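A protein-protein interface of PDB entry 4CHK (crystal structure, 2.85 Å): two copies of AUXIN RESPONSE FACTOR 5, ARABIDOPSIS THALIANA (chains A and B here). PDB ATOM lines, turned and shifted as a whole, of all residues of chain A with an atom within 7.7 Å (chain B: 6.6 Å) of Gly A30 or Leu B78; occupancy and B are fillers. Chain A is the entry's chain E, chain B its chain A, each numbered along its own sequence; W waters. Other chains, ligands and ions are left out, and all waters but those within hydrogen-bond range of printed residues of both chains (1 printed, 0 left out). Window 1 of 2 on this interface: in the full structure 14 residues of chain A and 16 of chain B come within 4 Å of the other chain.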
ATOM      1  N   THR A  21     -17.470   2.545 -16.735  1.00  0.00           N
ATOM      2  CA  THR A  21     -16.773   3.825 -16.570  1.00  0.00           C
ATOM      3  C   THR A  21     -16.715   4.224 -15.094  1.00  0.00           C
ATOM      4  O   THR A  21     -17.752   4.221 -14.418  1.00  0.00           O
ATOM      5  CB  THR A  21     -17.473   4.899 -17.445  1.00  0.00           C
ATOM      6  OG1 THR A  21     -17.438   4.496 -18.814  1.00  0.00           O
ATOM      7  CG2 THR A  21     -16.851   6.277 -17.319  1.00  0.00           C
ATOM      8  N   LYS A  22     -15.505   4.596 -14.611  1.00  0.00           N
ATOM      9  CA  LYS A  22     -15.251   5.047 -13.236  1.00  0.00           C
ATOM     10  C   LYS A  22     -15.885   6.385 -13.024  1.00  0.00           C
ATOM     11  O   LYS A  22     -15.841   7.224 -13.919  1.00  0.00           O
ATOM     12  CB  LYS A  22     -13.741   5.211 -12.955  1.00  0.00           C
ATOM     13  CG  LYS A  22     -12.973   3.923 -12.823  1.00  0.00           C
ATOM     14  CD  LYS A  22     -11.473   4.160 -12.679  1.00  0.00           C
ATOM     15  CE  LYS A  22     -10.739   2.836 -12.841  1.00  0.00           C
ATOM     16  NZ  LYS A  22      -9.266   2.930 -12.599  1.00  0.00           N
ATOM     17  N   VAL A  23     -16.465   6.599 -11.838  1.00  0.00           N
ATOM     18  CA  VAL A  23     -17.048   7.880 -11.411  1.00  0.00           C
ATOM     19  C   VAL A  23     -16.320   8.222 -10.128  1.00  0.00           C
ATOM     20  O   VAL A  23     -16.304   7.436  -9.158  1.00  0.00           O
ATOM     21  CB  VAL A  23     -18.576   7.868 -11.236  1.00  0.00           C
ATOM     22  CG1 VAL A  23     -19.073   9.258 -10.888  1.00  0.00           C
ATOM     23  CG2 VAL A  23     -19.260   7.368 -12.496  1.00  0.00           C
ATOM     24  N   GLN A  24     -15.647   9.365 -10.151  1.00  0.00           N
ATOM     25  CA  GLN A  24     -14.808   9.749  -9.033  1.00  0.00           C
ATOM     26  C   GLN A  24     -15.091  11.089  -8.357  1.00  0.00           C
ATOM     27  O   GLN A  24     -15.589  12.017  -8.976  1.00  0.00           O
ATOM     28  CB  GLN A  24     -13.350   9.602  -9.440  1.00  0.00           C
ATOM     29  CG  GLN A  24     -12.934   8.139  -9.545  1.00  0.00           C
ATOM     30  CD  GLN A  24     -11.654   7.996 -10.303  1.00  0.00           C
ATOM     31  OE1 GLN A  24     -11.449   8.607 -11.394  1.00  0.00           O
ATOM     32  NE2 GLN A  24     -10.755   7.210  -9.700  1.00  0.00           N
ATOM     33  N   LYS A  25     -14.805  11.155  -7.064  1.00  0.00           N
ATOM     34  CA  LYS A  25     -14.986  12.338  -6.248  1.00  0.00           C
ATOM     35  C   LYS A  25     -13.926  12.279  -5.171  1.00  0.00           C
ATOM     36  O   LYS A  25     -13.751  11.248  -4.528  1.00  0.00           O
ATOM     37  CB  LYS A  25     -16.400  12.408  -5.637  1.00  0.00           C
ATOM     38  CG  LYS A  25     -16.725  13.798  -5.096  1.00  0.00           C
ATOM     39  CD  LYS A  25     -17.965  13.841  -4.233  1.00  0.00           C
ATOM     40  CE  LYS A  25     -17.725  14.721  -3.037  1.00  0.00           C
ATOM     41  NZ  LYS A  25     -16.975  14.002  -1.953  1.00  0.00           N
ATOM     42  N   GLY A  27     -12.147  12.456  -1.853  1.00  0.00           N
ATOM     43  CA  GLY A  27     -12.558  12.215  -0.474  1.00  0.00           C
ATOM     44  C   GLY A  27     -13.703  11.234  -0.428  1.00  0.00           C
ATOM     45  O   GLY A  27     -14.257  10.975   0.640  1.00  0.00           O
ATOM     46  N   SER A  28     -14.037  10.650  -1.589  1.00  0.00           N
ATOM     47  CA  SER A  28     -15.076   9.649  -1.722  1.00  0.00           C
ATOM     48  C   SER A  28     -14.543   8.400  -2.413  1.00  0.00           C
ATOM     49  O   SER A  28     -13.624   8.497  -3.239  1.00  0.00           O
ATOM     50  CB  SER A  28     -16.253  10.207  -2.500  1.00  0.00           C
ATOM     51  OG  SER A  28     -16.886  11.197  -1.715  1.00  0.00           O
ATOM     52  N   VAL A  29     -15.100   7.217  -2.038  1.00  0.00           N
ATOM     53  CA  VAL A  29     -14.810   5.918  -2.633  1.00  0.00           C
ATOM     54  C   VAL A  29     -15.389   6.021  -4.038  1.00  0.00           C
ATOM     55  O   VAL A  29     -16.534   6.461  -4.202  1.00  0.00           O
ATOM     56  CB  VAL A  29     -15.460   4.756  -1.818  1.00  0.00           C
ATOM     57  CG1 VAL A  29     -15.488   3.440  -2.603  1.00  0.00           C
ATOM     58  CG2 VAL A  29     -14.769   4.580  -0.470  1.00  0.00           C
ATOM     59  N   GLY A  30     -14.571   5.672  -5.028  1.00  0.00           N
ATOM     60  CA  GLY A  30     -14.942   5.695  -6.435  1.00  0.00           C
ATOM     61  C   GLY A  30     -16.017   4.694  -6.778  1.00  0.00           C
ATOM     62  O   GLY A  30     -16.343   3.812  -5.966  1.00  0.00           O
ATOM     63  N   ARG A  31     -16.606   4.855  -7.983  1.00  0.00           N
ATOM     64  CA  ARG A  31     -17.665   3.967  -8.466  1.00  0.00           C
ATOM     65  C   ARG A  31     -17.393   3.546  -9.909  1.00  0.00           C
ATOM     66  O   ARG A  31     -16.427   4.005 -10.507  1.00  0.00           O
ATOM     67  CB  ARG A  31     -19.051   4.643  -8.344  1.00  0.00           C
ATOM     68  CG  ARG A  31     -19.528   4.925  -6.931  1.00  0.00           C
ATOM     69  CD  ARG A  31     -19.801   3.670  -6.128  1.00  0.00           C
ATOM     70  NE  ARG A  31     -21.152   3.687  -5.578  1.00  0.00           N
ATOM     71  CZ  ARG A  31     -22.048   2.738  -5.805  1.00  0.00           C
ATOM     72  NH1 ARG A  31     -21.747   1.701  -6.564  1.00  0.00           N
ATOM     73  NH2 ARG A  31     -23.259   2.818  -5.267  1.00  0.00           N
ATOM     74  N   SER A  32     -18.233   2.657 -10.451  1.00  0.00           N
ATOM     75  CA  SER A  32     -18.161   2.202 -11.831  1.00  0.00           C
ATOM     76  C   SER A  32     -19.598   2.048 -12.354  1.00  0.00           C
ATOM     77  O   SER A  32     -20.429   1.415 -11.690  1.00  0.00           O
ATOM     78  CB  SER A  32     -17.365   0.902 -11.947  1.00  0.00           C
ATOM     79  OG  SER A  32     -16.021   1.124 -12.355  1.00  0.00           O
ATOM     80  N   MET A  51     -25.724   8.151  -6.076  1.00  0.00           N
ATOM     81  CA  MET A  51     -24.522   7.395  -5.741  1.00  0.00           C
ATOM     82  C   MET A  51     -23.567   8.109  -4.798  1.00  0.00           C
ATOM     83  O   MET A  51     -22.837   7.434  -4.054  1.00  0.00           O
ATOM     84  CB  MET A  51     -23.755   7.107  -7.033  1.00  0.00           C
ATOM     85  CG  MET A  51     -24.151   5.835  -7.685  1.00  0.00           C
ATOM     86  SD  MET A  51     -23.314   5.723  -9.265  1.00  0.00           S
ATOM     87  CE  MET A  51     -22.617   4.183  -9.108  1.00  0.00           C
ATOM     88  N   PHE A  52     -23.485   9.458  -4.916  1.00  0.00           N
ATOM     89  CA  PHE A  52     -22.586  10.316  -4.141  1.00  0.00           C
ATOM     90  C   PHE A  52     -23.299  11.342  -3.214  1.00  0.00           C
ATOM     91  O   PHE A  52     -22.619  12.132  -2.549  1.00  0.00           O
ATOM     92  CB  PHE A  52     -21.570  10.993  -5.074  1.00  0.00           C
ATOM     93  CG  PHE A  52     -20.561  10.073  -5.731  1.00  0.00           C
ATOM     94  CD1 PHE A  52     -19.339   9.804  -5.119  1.00  0.00           C
ATOM     95  CD2 PHE A  52     -20.809   9.521  -6.980  1.00  0.00           C
ATOM     96  CE1 PHE A  52     -18.399   8.980  -5.731  1.00  0.00           C
ATOM     97  CE2 PHE A  52     -19.865   8.704  -7.592  1.00  0.00           C
ATOM     98  CZ  PHE A  52     -18.660   8.455  -6.970  1.00  0.00           C
ATOM     99  N   LEU B  68     -16.769  -2.272   1.691  1.00  0.00           N
ATOM    100  CA  LEU B  68     -15.673  -3.131   1.275  1.00  0.00           C
ATOM    101  C   LEU B  68     -15.140  -2.477  -0.020  1.00  0.00           C
ATOM    102  O   LEU B  68     -15.834  -2.448  -1.050  1.00  0.00           O
ATOM    103  CB  LEU B  68     -16.093  -4.611   1.057  1.00  0.00           C
ATOM    104  CG  LEU B  68     -14.982  -5.518   0.545  1.00  0.00           C
ATOM    105  CD1 LEU B  68     -14.099  -5.988   1.652  1.00  0.00           C
ATOM    106  CD2 LEU B  68     -15.536  -6.670  -0.182  1.00  0.00           C
ATOM    107  N   VAL B  69     -13.951  -1.883   0.075  1.00  0.00           N
ATOM    108  CA  VAL B  69     -13.323  -1.212  -1.067  1.00  0.00           C
ATOM    109  C   VAL B  69     -12.127  -1.961  -1.589  1.00  0.00           C
ATOM    110  O   VAL B  69     -11.713  -2.936  -0.960  1.00  0.00           O
ATOM    111  CB  VAL B  69     -13.015   0.262  -0.814  1.00  0.00           C
ATOM    112  CG1 VAL B  69     -14.274   0.982  -0.422  1.00  0.00           C
ATOM    113  CG2 VAL B  69     -11.966   0.426   0.257  1.00  0.00           C
ATOM    114  N   TYR B  70     -11.588  -1.521  -2.758  1.00  0.00           N
ATOM    115  CA  TYR B  70     -10.386  -2.091  -3.380  1.00  0.00           C
ATOM    116  C   TYR B  70      -9.567  -1.059  -4.129  1.00  0.00           C
ATOM    117  O   TYR B  70     -10.089  -0.013  -4.534  1.00  0.00           O
ATOM    118  CB  TYR B  70     -10.669  -3.353  -4.240  1.00  0.00           C
ATOM    119  CG  TYR B  70     -11.182  -3.113  -5.648  1.00  0.00           C
ATOM    120  CD1 TYR B  70     -12.532  -2.879  -5.889  1.00  0.00           C
ATOM    121  CD2 TYR B  70     -10.329  -3.199  -6.747  1.00  0.00           C
ATOM    122  CE1 TYR B  70     -13.015  -2.684  -7.184  1.00  0.00           C
ATOM    123  CE2 TYR B  70     -10.799  -2.996  -8.046  1.00  0.00           C
ATOM    124  CZ  TYR B  70     -12.141  -2.725  -8.257  1.00  0.00           C
ATOM    125  OH  TYR B  70     -12.614  -2.529  -9.535  1.00  0.00           O
ATOM    126  N   VAL B  71      -8.266  -1.329  -4.261  1.00  0.00           N
ATOM    127  CA  VAL B  71      -7.364  -0.479  -5.031  1.00  0.00           C
ATOM    128  C   VAL B  71      -7.105  -1.232  -6.332  1.00  0.00           C
ATOM    129  O   VAL B  71      -6.846  -2.429  -6.292  1.00  0.00           O
ATOM    130  CB  VAL B  71      -6.051  -0.065  -4.292  1.00  0.00           C
ATOM    131  CG1 VAL B  71      -5.119   0.700  -5.219  1.00  0.00           C
ATOM    132  CG2 VAL B  71      -6.354   0.769  -3.051  1.00  0.00           C
ATOM    133  N   ASP B  72      -7.242  -0.557  -7.474  1.00  0.00           N
ATOM    134  CA  ASP B  72      -6.993  -1.191  -8.754  1.00  0.00           C
ATOM    135  C   ASP B  72      -5.597  -0.864  -9.337  1.00  0.00           C
ATOM    136  O   ASP B  72      -4.796  -0.130  -8.724  1.00  0.00           O
ATOM    137  CB  ASP B  72      -8.165  -0.963  -9.732  1.00  0.00           C
ATOM    138  CG  ASP B  72      -8.244   0.344 -10.504  1.00  0.00           C
ATOM    139  OD1 ASP B  72      -7.613   1.345 -10.075  1.00  0.00           O
ATOM    140  OD2 ASP B  72      -8.945   0.376 -11.526  1.00  0.00           O
ATOM    141  N   ASP B  76      -6.722   3.511  -7.911  1.00  0.00           N
ATOM    142  CA  ASP B  76      -8.021   4.091  -7.617  1.00  0.00           C
ATOM    143  C   ASP B  76      -8.773   3.245  -6.591  1.00  0.00           C
ATOM    144  O   ASP B  76      -8.853   2.019  -6.727  1.00  0.00           O
ATOM    145  CB  ASP B  76      -8.845   4.242  -8.923  1.00  0.00           C
ATOM    146  CG  ASP B  76      -8.341   5.300  -9.913  1.00  0.00           C
ATOM    147  OD1 ASP B  76      -8.068   6.443  -9.479  1.00  0.00           O
ATOM    148  OD2 ASP B  76      -8.363   5.029 -11.137  1.00  0.00           O
ATOM    149  N   VAL B  77      -9.307   3.919  -5.548  1.00  0.00           N
ATOM    150  CA  VAL B  77     -10.108   3.300  -4.483  1.00  0.00           C
ATOM    151  C   VAL B  77     -11.532   3.264  -5.022  1.00  0.00           C
ATOM    152  O   VAL B  77     -12.114   4.312  -5.320  1.00  0.00           O
ATOM    153  CB  VAL B  77     -10.028   4.057  -3.138  1.00  0.00           C
ATOM    154  CG1 VAL B  77     -11.001   3.466  -2.109  1.00  0.00           C
ATOM    155  CG2 VAL B  77      -8.597   4.095  -2.598  1.00  0.00           C
ATOM    156  N   LEU B  78     -12.048   2.044  -5.209  1.00  0.00           N
ATOM    157  CA  LEU B  78     -13.345   1.765  -5.781  1.00  0.00           C
ATOM    158  C   LEU B  78     -14.085   0.810  -4.851  1.00  0.00           C
ATOM    159  O   LEU B  78     -13.451   0.001  -4.164  1.00  0.00           O
ATOM    160  CB  LEU B  78     -13.166   1.100  -7.170  1.00  0.00           C
ATOM    161  CG  LEU B  78     -12.427   1.850  -8.279  1.00  0.00           C
ATOM    162  CD1 LEU B  78     -11.974   0.917  -9.347  1.00  0.00           C
ATOM    163  CD2 LEU B  78     -13.268   2.938  -8.877  1.00  0.00           C
ATOM    164  N   LEU B  79     -15.433   0.870  -4.879  1.00  0.00           N
ATOM    165  CA  LEU B  79     -16.336   0.018  -4.100  1.00  0.00           C
ATOM    166  C   LEU B  79     -16.431  -1.356  -4.726  1.00  0.00           C
ATOM    167  O   LEU B  79     -16.633  -1.449  -5.931  1.00  0.00           O
ATOM    168  CB  LEU B  79     -17.737   0.648  -4.065  1.00  0.00           C
ATOM    169  CG  LEU B  79     -18.769  -0.048  -3.210  1.00  0.00           C
ATOM    170  CD1 LEU B  79     -18.677   0.405  -1.765  1.00  0.00           C
ATOM    171  CD2 LEU B  79     -20.135   0.175  -3.763  1.00  0.00           C
ATOM    172  N   VAL B  80     -16.341  -2.417  -3.913  1.00  0.00           N
ATOM    173  CA  VAL B  80     -16.450  -3.784  -4.410  1.00  0.00           C
ATOM    174  C   VAL B  80     -17.901  -4.094  -4.761  1.00  0.00           C
ATOM    175  O   VAL B  80     -18.771  -4.072  -3.865  1.00  0.00           O
ATOM    176  CB  VAL B  80     -15.849  -4.845  -3.461  1.00  0.00           C
ATOM    177  CG1 VAL B  80     -16.173  -6.241  -3.952  1.00  0.00           C
ATOM    178  CG2 VAL B  80     -14.346  -4.683  -3.340  1.00  0.00           C
ATOM    179  N   ASP B  82     -19.525  -3.141  -8.208  1.00  0.00           N
ATOM    180  CA  ASP B  82     -19.877  -2.422  -9.424  1.00  0.00           C
ATOM    181  C   ASP B  82     -19.566  -3.066 -10.752  1.00  0.00           C
ATOM    182  O   ASP B  82     -20.401  -3.027 -11.651  1.00  0.00           O
ATOM    183  CB  ASP B  82     -19.287  -1.005  -9.378  1.00  0.00           C
ATOM    184  CG  ASP B  82     -19.865  -0.113  -8.308  1.00  0.00           C
ATOM    185  OD1 ASP B  82     -20.847  -0.526  -7.656  1.00  0.00           O
ATOM    186  OD2 ASP B  82     -19.355   1.012  -8.136  1.00  0.00           O
ATOM    187  N   ASP B  83     -18.368  -3.594 -10.907  1.00  0.00           N
ATOM    188  CA  ASP B  83     -17.907  -4.168 -12.165  1.00  0.00           C
ATOM    189  C   ASP B  83     -18.350  -5.646 -12.456  1.00  0.00           C
ATOM    190  O   ASP B  83     -18.665  -6.398 -11.523  1.00  0.00           O
ATOM    191  CB  ASP B  83     -16.370  -4.093 -12.174  1.00  0.00           C
ATOM    192  CG  ASP B  83     -15.857  -2.692 -12.014  1.00  0.00           C
ATOM    193  OD1 ASP B  83     -15.854  -1.946 -13.032  1.00  0.00           O
ATOM    194  OD2 ASP B  83     -15.509  -2.307 -10.851  1.00  0.00           O
ATOM    195  N   CYS B  91      -8.391  -6.388 -12.434  1.00  0.00           N
ATOM    196  CA  CYS B  91      -8.043  -5.040 -11.952  1.00  0.00           C
ATOM    197  C   CYS B  91      -7.600  -4.946 -10.517  1.00  0.00           C
ATOM    198  O   CYS B  91      -6.751  -4.115 -10.200  1.00  0.00           O
ATOM    199  CB  CYS B  91      -9.192  -4.086 -12.217  1.00  0.00           C
ATOM    200  SG  CYS B  91      -9.681  -4.024 -13.954  1.00  0.00           S
ATOM    201  N   MET B 106     -11.796   9.689   5.509  1.00  0.00           N
ATOM    202  CA  MET B 106     -11.421   9.773   4.101  1.00  0.00           C
ATOM    203  C   MET B 106     -11.899  11.121   3.480  1.00  0.00           C
ATOM    204  O   MET B 106     -11.184  11.751   2.680  1.00  0.00           O
ATOM    205  CB  MET B 106     -12.064   8.564   3.387  1.00  0.00           C
ATOM    206  CG  MET B 106     -11.792   8.489   1.931  1.00  0.00           C
ATOM    207  SD  MET B 106     -12.104   6.866   1.187  1.00  0.00           S
ATOM    208  CE  MET B 106     -12.009   7.383  -0.515  1.00  0.00           C
HETATM  209  O   HOH W   1     -11.562   6.597  -6.721  1.00  0.00           O
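Of the 14 printed residues of chain B, 9 touch a printed residue of chain A. Hydrophobic or aromatic side chains of chain B within 4 Å of the printed part of chain A: Val B69, Leu B78, Leu B79 and Met B106. Hydrophobic or aromatic side chains of chain A within 4 Å of the printed part of chain B: Val A29. Among the printed residues, 18 pairs touch across the chains. Among the printed residues, Asp or Glu carboxylates within 4 Å of a Lys or Arg side-chain nitrogen of the other chain: Lys A22 with Asp B72, Lys A22 with Asp B76 and Arg A31 with Asp B82.
Of the printed residues of chain B, Lys A22 touches Asp B72 and Asp B76. Printed residues of chain A within 4 Å of Asp B72: Lys A22 (2.8 Å). Printed residues of chain A within 4 Å of Asp B76: Lys A22 (2.7 Å) and Gln A24 (2.8 Å). Leu B78 touches just these residues of chain A: Val A29 (3.7 Å), Gly A30 (3.6 Å) and Arg A31 (3.7 Å). Of the printed residues of chain A, Leu B79 touches Val A29 (3.4 Å), Gly A30 (3.3 Å) and Arg A31 (3.6 Å). Printed residues of chain A within 4 Å of Met B106: Gly A27 (3.5 Å), Ser A28 (3.3 Å) and Val A29 (3.4 Å). The nearest residue of chain B that does not touch Gly A30 is Asp B82 (4.6 Å). The nearest printed residue of chain B that does not touch Ser A28 is Val B77 (4.9 Å).
The side-chain hydroxyl (OG) of Ser A28 sits at hydrogen-bond distance from the side-chain amino group (NZ) of Lys A25, at 2.8 Å. N of Arg A31 lies within hydrogen-bond range of O of Val A23 (2.9 Å). The side-chain carboxylate (OD2) of Asp B83 is in hydrogen-bond range of the side-chain hydroxyl (OH) of Tyr B70, at 3.2 Å. The side-chain carboxylate of Asp B72 is in hydrogen-bond range of the backbone NH of Asp B76, 3.2 Å away. The backbone NH (N) of Tyr B70 lies within hydrogen-bond range of the backbone carbonyl oxygen (O) of Leu B78, at 2.8 Å.
Among the printed residues, merely in contact across the chains: Ser A28 with Met B106, Val A29 with Leu B79, Val A29 with Met B106, Gly A27 with Met B106, Val A29 with Val B69, Arg A31 with Leu B79, Gly A30 with Leu B78, Arg A31 with Leu B78, Val A29 with Leu B78 and Val A29 with Val B77.
O of Val B77 sits at hydrogen-bond distance from N of Gly A30 (2.8 Å). The side-chain amino group of Lys A22 lies within salt-bridge range of the side-chain carboxylate of Asp B76, 2.7 Å away. NH1 of Arg A31 is in salt-bridge range of OD1 of Asp B82, 2.6 Å away. The side-chain carboxylate of Asp B82 is in hydrogen-bond range of the backbone NH of Ser A32 (3.1 Å). OG of Ser A32 lies within hydrogen-bond range of OD1 of Asp B83, 3.1 Å away. The backbone NH (N) of Leu B79 sits at hydrogen-bond distance from the backbone carbonyl oxygen (O) of Gly A30 (3.3 Å). The side-chain amino group (NZ) of Lys A22 lies within salt-bridge range of the side-chain carboxylate (OD2) of Asp B72. OD1 of Asp B76 lies within hydrogen-bond range of NE2 of Gln A24, 2.8 Å away.
Water W1 bridges the backbone carbonyl oxygen (O) of Val B77 and the side-chain amide nitrogen (NE2) of Gln A24.
No position is printed for both chains. Of the 18 pairs that touch across the chains among the printed residues, none has its exchanged pair printed and touching as well.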
